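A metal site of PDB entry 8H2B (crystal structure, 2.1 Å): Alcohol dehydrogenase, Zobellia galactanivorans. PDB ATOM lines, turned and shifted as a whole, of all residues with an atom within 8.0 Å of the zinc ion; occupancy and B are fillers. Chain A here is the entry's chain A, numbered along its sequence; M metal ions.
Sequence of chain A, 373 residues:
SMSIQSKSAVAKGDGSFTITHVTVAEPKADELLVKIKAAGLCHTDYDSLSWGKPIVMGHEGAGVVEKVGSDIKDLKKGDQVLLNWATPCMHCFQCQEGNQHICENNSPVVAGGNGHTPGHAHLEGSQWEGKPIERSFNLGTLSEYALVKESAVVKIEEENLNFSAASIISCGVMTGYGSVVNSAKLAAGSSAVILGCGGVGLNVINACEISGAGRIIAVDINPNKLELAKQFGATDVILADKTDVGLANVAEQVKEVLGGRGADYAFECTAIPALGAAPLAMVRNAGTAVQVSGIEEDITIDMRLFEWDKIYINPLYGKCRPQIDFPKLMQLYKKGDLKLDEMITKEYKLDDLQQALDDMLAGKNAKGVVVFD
The zinc ion is bound by the side-chain sulfur of Cys 95 (2.3 Å), the side-chain sulfur of Cys 103 (2.3 Å), the side-chain sulfur of Cys 92 (2.3 Å) and the side-chain sulfur of Cys 89 (2.4 Å). The zinc ion has four donor atoms within binding distance.
Met 90 touches the zinc ion (N to ZN, 3.8 Å). Five residues have an atom within 4 Å of the zinc ion: Cys 89, Met 90, Cys 92, Cys 95 and Cys 103. Along chain A the residues within 4 Å of the zinc ion span positions 89 to 103. The nearest printed residue that does not touch the zinc ion is Glu 104 (4.05 Å).
The side-chain sulfur (SG) of Cys 95 lies close to the backbone NH (N) of Met 90 (3.3 Å). The side-chain sulfur of Cys 103 lies close to the backbone NH of Asn 105. The side-chain sulfur (SG) of Cys 103 sits close to the backbone NH (N) of Asn 106 (3.4 Å). The side-chain sulfur of Cys 92 sits close to the backbone NH of Glu 104 (3.3 Å). The backbone NH of Gln 94 lies close to the side-chain sulfur of Cys 92 (3.6 Å). The backbone NH of His 91 sits close to the side-chain sulfur of Cys 89. SG of Cys 89 sits close to ND2 of Asn 105 (3.6 Å).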
ATOM      1  N   ALA A  86      12.649   4.342  11.416  1.00  0.00           N
ATOM      2  CA  ALA A  86      12.669   3.309  12.448  1.00  0.00           C
ATOM      3  C   ALA A  86      13.753   3.605  13.486  1.00  0.00           C
ATOM      4  O   ALA A  86      13.514   3.434  14.684  1.00  0.00           O
ATOM      5  CB  ALA A  86      12.865   1.932  11.822  1.00  0.00           C
ATOM      6  N   THR A  87      14.901   4.119  13.042  1.00  0.00           N
ATOM      7  CA  THR A  87      16.112   4.343  13.840  1.00  0.00           C
ATOM      8  C   THR A  87      16.265   3.256  14.909  1.00  0.00           C
ATOM      9  O   THR A  87      16.297   3.564  16.100  1.00  0.00           O
ATOM     10  CB  THR A  87      16.108   5.734  14.506  1.00  0.00           C
ATOM     11  OG1 THR A  87      14.938   5.890  15.336  1.00  0.00           O
ATOM     12  CG2 THR A  87      16.101   6.846  13.469  1.00  0.00           C
ATOM     13  N   PRO A  88      16.341   1.971  14.516  1.00  0.00           N
ATOM     14  CA  PRO A  88      16.165   0.895  15.505  1.00  0.00           C
ATOM     15  C   PRO A  88      17.389   0.682  16.398  1.00  0.00           C
ATOM     16  O   PRO A  88      18.530   0.930  16.004  1.00  0.00           O
ATOM     17  CB  PRO A  88      15.916  -0.320  14.618  1.00  0.00           C
ATOM     18  CG  PRO A  88      16.686   0.014  13.313  1.00  0.00           C
ATOM     19  CD  PRO A  88      16.539   1.481  13.137  1.00  0.00           C
ATOM     20  N   CYS A  89      17.134   0.170  17.617  1.00  0.00           N
ATOM     21  CA  CYS A  89      18.207   0.009  18.610  1.00  0.00           C
ATOM     22  C   CYS A  89      19.019  -1.267  18.406  1.00  0.00           C
ATOM     23  O   CYS A  89      20.179  -1.304  18.806  1.00  0.00           O
ATOM     24  CB  CYS A  89      17.646   0.057  20.048  1.00  0.00           C
ATOM     25  SG  CYS A  89      16.931  -1.499  20.728  1.00  0.00           S
ATOM     26  N   MET A  90      18.422  -2.313  17.837  1.00  0.00           N
ATOM     27  CA  MET A  90      19.072  -3.561  17.415  1.00  0.00           C
ATOM     28  C   MET A  90      19.228  -4.537  18.581  1.00  0.00           C
ATOM     29  O   MET A  90      19.714  -5.664  18.364  1.00  0.00           O
ATOM     30  CB  MET A  90      20.434  -3.312  16.727  1.00  0.00           C
ATOM     31  CG  MET A  90      20.263  -2.471  15.453  1.00  0.00           C
ATOM     32  SD  MET A  90      19.372  -3.376  14.205  1.00  0.00           S
ATOM     33  CE  MET A  90      17.749  -2.857  14.430  1.00  0.00           C
ATOM     34  N   HIS A  91      18.792  -4.171  19.802  1.00  0.00           N
ATOM     35  CA  HIS A  91      18.962  -5.025  20.981  1.00  0.00           C
ATOM     36  C   HIS A  91      17.682  -5.322  21.755  1.00  0.00           C
ATOM     37  O   HIS A  91      17.678  -6.294  22.524  1.00  0.00           O
ATOM     38  CB  HIS A  91      19.984  -4.406  21.943  1.00  0.00           C
ATOM     39  CG  HIS A  91      21.395  -4.588  21.490  1.00  0.00           C
ATOM     40  ND1 HIS A  91      21.998  -3.757  20.562  1.00  0.00           N
ATOM     41  CD2 HIS A  91      22.312  -5.539  21.799  1.00  0.00           C
ATOM     42  CE1 HIS A  91      23.230  -4.187  20.344  1.00  0.00           C
ATOM     43  NE2 HIS A  91      23.444  -5.256  21.079  1.00  0.00           N
ATOM     44  N   CYS A  92      16.603  -4.560  21.580  1.00  0.00           N
ATOM     45  CA  CYS A  92      15.409  -4.792  22.371  1.00  0.00           C
ATOM     46  C   CYS A  92      14.687  -6.049  21.864  1.00  0.00           C
ATOM     47  O   CYS A  92      15.073  -6.638  20.859  1.00  0.00           O
ATOM     48  CB  CYS A  92      14.465  -3.581  22.310  1.00  0.00           C
ATOM     49  SG  CYS A  92      13.594  -3.421  20.700  1.00  0.00           S
ATOM     50  N   PHE A  93      13.659  -6.466  22.601  1.00  0.00           N
ATOM     51  CA  PHE A  93      12.906  -7.657  22.239  1.00  0.00           C
ATOM     52  C   PHE A  93      12.379  -7.591  20.804  1.00  0.00           C
ATOM     53  O   PHE A  93      12.537  -8.540  20.029  1.00  0.00           O
ATOM     54  CB  PHE A  93      11.750  -7.855  23.215  1.00  0.00           C
ATOM     55  CG  PHE A  93      10.813  -8.943  22.807  1.00  0.00           C
ATOM     56  CD1 PHE A  93      11.148 -10.279  23.000  1.00  0.00           C
ATOM     57  CD2 PHE A  93       9.591  -8.650  22.207  1.00  0.00           C
ATOM     58  CE1 PHE A  93      10.287 -11.298  22.600  1.00  0.00           C
ATOM     59  CE2 PHE A  93       8.730  -9.668  21.807  1.00  0.00           C
ATOM     60  CZ  PHE A  93       9.078 -10.992  22.014  1.00  0.00           C
ATOM     61  N   GLN A  94      11.751  -6.482  20.449  1.00  0.00           N
ATOM     62  CA  GLN A  94      11.176  -6.363  19.113  1.00  0.00           C
ATOM     63  C   GLN A  94      12.268  -6.374  18.035  1.00  0.00           C
ATOM     64  O   GLN A  94      12.122  -7.071  17.022  1.00  0.00           O
ATOM     65  CB  GLN A  94      10.293  -5.124  19.023  1.00  0.00           C
ATOM     66  CG  GLN A  94       8.977  -5.237  19.819  1.00  0.00           C
ATOM     67  CD  GLN A  94       8.017  -6.332  19.289  1.00  0.00           C
ATOM     68  OE1 GLN A  94       8.307  -7.051  18.322  1.00  0.00           O
ATOM     69  NE2 GLN A  94       6.874  -6.475  19.959  1.00  0.00           N
ATOM     70  N   CYS A  95      13.378  -5.655  18.244  1.00  0.00           N
ATOM     71  CA  CYS A  95      14.477  -5.713  17.277  1.00  0.00           C
ATOM     72  C   CYS A  95      14.986  -7.145  17.101  1.00  0.00           C
ATOM     73  O   CYS A  95      15.316  -7.569  15.987  1.00  0.00           O
ATOM     74  CB  CYS A  95      15.618  -4.790  17.699  1.00  0.00           C
ATOM     75  SG  CYS A  95      15.238  -3.034  17.382  1.00  0.00           S
ATOM     76  N   GLN A  96      15.047  -7.909  18.190  1.00  0.00           N
ATOM     77  CA  GLN A  96      15.574  -9.271  18.052  1.00  0.00           C
ATOM     78  C   GLN A  96      14.575 -10.211  17.400  1.00  0.00           C
ATOM     79  O   GLN A  96      14.974 -11.267  16.906  1.00  0.00           O
ATOM     80  CB  GLN A  96      16.006  -9.792  19.427  1.00  0.00           C
ATOM     81  CG  GLN A  96      17.230  -9.024  19.945  1.00  0.00           C
ATOM     82  CD  GLN A  96      17.972  -9.788  21.025  1.00  0.00           C
ATOM     83  OE1 GLN A  96      18.204 -10.987  20.893  1.00  0.00           O
ATOM     84  NE2 GLN A  96      18.363  -9.083  22.085  1.00  0.00           N
ATOM     85  N   ASN A  99      11.536  -7.186  14.301  1.00  0.00           N
ATOM     86  CA  ASN A  99      10.549  -6.111  14.208  1.00  0.00           C
ATOM     87  C   ASN A  99      11.177  -4.762  14.531  1.00  0.00           C
ATOM     88  O   ASN A  99      10.847  -4.093  15.505  1.00  0.00           O
ATOM     89  CB  ASN A  99       9.375  -6.420  15.136  1.00  0.00           C
ATOM     90  CG  ASN A  99       8.574  -7.626  14.674  1.00  0.00           C
ATOM     91  OD1 ASN A  99       8.408  -7.853  13.459  1.00  0.00           O
ATOM     92  ND2 ASN A  99       8.076  -8.401  15.615  1.00  0.00           N
ATOM     93  N   GLN A 100      12.145  -4.385  13.685  1.00  0.00           N
ATOM     94  CA  GLN A 100      12.881  -3.141  13.883  1.00  0.00           C
ATOM     95  C   GLN A 100      11.964  -1.919  13.832  1.00  0.00           C
ATOM     96  O   GLN A 100      12.256  -0.867  14.425  1.00  0.00           O
ATOM     97  CB  GLN A 100      13.955  -3.032  12.808  1.00  0.00           C
ATOM     98  CG  GLN A 100      15.022  -4.117  12.942  1.00  0.00           C
ATOM     99  CD  GLN A 100      16.130  -3.976  11.922  1.00  0.00           C
ATOM    100  OE1 GLN A 100      16.354  -2.885  11.351  1.00  0.00           O
ATOM    101  NE2 GLN A 100      16.882  -5.063  11.713  1.00  0.00           N
ATOM    102  N   HIS A 101      10.860  -2.046  13.111  1.00  0.00           N
ATOM    103  CA  HIS A 101       9.925  -0.962  12.900  1.00  0.00           C
ATOM    104  C   HIS A 101       9.057  -0.679  14.117  1.00  0.00           C
ATOM    105  O   HIS A 101       8.351   0.328  14.137  1.00  0.00           O
ATOM    106  CB  HIS A 101       9.060  -1.341  11.703  1.00  0.00           C
ATOM    107  CG  HIS A 101       8.286  -2.596  11.939  1.00  0.00           C
ATOM    108  ND1 HIS A 101       8.893  -3.831  12.021  1.00  0.00           N
ATOM    109  CD2 HIS A 101       6.969  -2.801  12.159  1.00  0.00           C
ATOM    110  CE1 HIS A 101       7.970  -4.747  12.280  1.00  0.00           C
ATOM    111  NE2 HIS A 101       6.790  -4.147  12.353  1.00  0.00           N
ATOM    112  N   ILE A 102       9.069  -1.557  15.126  1.00  0.00           N
ATOM    113  CA  ILE A 102       8.389  -1.238  16.389  1.00  0.00           C
ATOM    114  C   ILE A 102       9.381  -1.365  17.542  1.00  0.00           C
ATOM    115  O   ILE A 102       9.043  -1.885  18.615  1.00  0.00           O
ATOM    116  CB  ILE A 102       7.161  -2.135  16.591  1.00  0.00           C
ATOM    117  CG1 ILE A 102       7.485  -3.572  16.205  1.00  0.00           C
ATOM    118  CG2 ILE A 102       5.992  -1.628  15.744  1.00  0.00           C
ATOM    119  CD1 ILE A 102       6.406  -4.579  16.654  1.00  0.00           C
ATOM    120  N   CYS A 103      10.605  -0.893  17.327  1.00  0.00           N
ATOM    121  CA  CYS A 103      11.643  -0.936  18.341  1.00  0.00           C
ATOM    122  C   CYS A 103      11.165  -0.296  19.637  1.00  0.00           C
ATOM    123  O   CYS A 103      10.674   0.841  19.644  1.00  0.00           O
ATOM    124  CB  CYS A 103      12.869  -0.216  17.798  1.00  0.00           C
ATOM    125  SG  CYS A 103      14.109   0.141  19.083  1.00  0.00           S
ATOM    126  N   GLU A 104      11.266  -1.038  20.750  1.00  0.00           N
ATOM    127  CA  GLU A 104      10.681  -0.578  22.015  1.00  0.00           C
ATOM    128  C   GLU A 104      11.422   0.614  22.601  1.00  0.00           C
ATOM    129  O   GLU A 104      10.874   1.288  23.470  1.00  0.00           O
ATOM    130  CB  GLU A 104      10.642  -1.718  23.033  1.00  0.00           C
ATOM    131  CG  GLU A 104       9.624  -2.814  22.698  1.00  0.00           C
ATOM    132  CD  GLU A 104       9.766  -4.059  23.588  1.00  0.00           C
ATOM    133  OE1 GLU A 104       8.896  -4.952  23.504  1.00  0.00           O
ATOM    134  OE2 GLU A 104      10.745  -4.156  24.353  1.00  0.00           O
ATOM    135  N   ASN A 105      12.630   0.911  22.147  1.00  0.00           N
ATOM    136  CA  ASN A 105      13.412   1.992  22.753  1.00  0.00           C
ATOM    137  C   ASN A 105      13.421   3.253  21.917  1.00  0.00           C
ATOM    138  O   ASN A 105      13.324   4.342  22.465  1.00  0.00           O
ATOM    139  CB  ASN A 105      14.865   1.559  22.988  1.00  0.00           C
ATOM    140  CG  ASN A 105      14.988   0.594  24.118  1.00  0.00           C
ATOM    141  OD1 ASN A 105      14.372   0.796  25.164  1.00  0.00           O
ATOM    142  ND2 ASN A 105      15.737  -0.483  23.918  1.00  0.00           N
ATOM    143  N   ASN A 106      13.547   3.105  20.591  1.00  0.00           N
ATOM    144  CA  ASN A 106      13.869   4.207  19.709  1.00  0.00           C
ATOM    145  C   ASN A 106      12.752   4.612  18.744  1.00  0.00           C
ATOM    146  O   ASN A 106      12.872   5.662  18.110  1.00  0.00           O
ATOM    147  CB  ASN A 106      15.103   3.837  18.857  1.00  0.00           C
ATOM    148  CG  ASN A 106      16.377   3.766  19.657  1.00  0.00           C
ATOM    149  OD1 ASN A 106      16.365   3.829  20.894  1.00  0.00           O
ATOM    150  ND2 ASN A 106      17.491   3.611  18.956  1.00  0.00           N
ATOM    151  N   SER A 107      11.733   3.786  18.569  1.00  0.00           N
ATOM    152  CA  SER A 107      10.690   4.111  17.581  1.00  0.00           C
ATOM    153  C   SER A 107      10.019   5.434  17.911  1.00  0.00           C
ATOM    154  O   SER A 107       9.442   5.564  19.010  1.00  0.00           O
ATOM    155  CB  SER A 107       9.611   3.053  17.519  1.00  0.00           C
ATOM    156  OG  SER A 107       8.496   3.581  16.812  1.00  0.00           O
HETATM  157 ZN    ZN M   1      14.976  -1.997  19.451  1.00  0.00          ZN
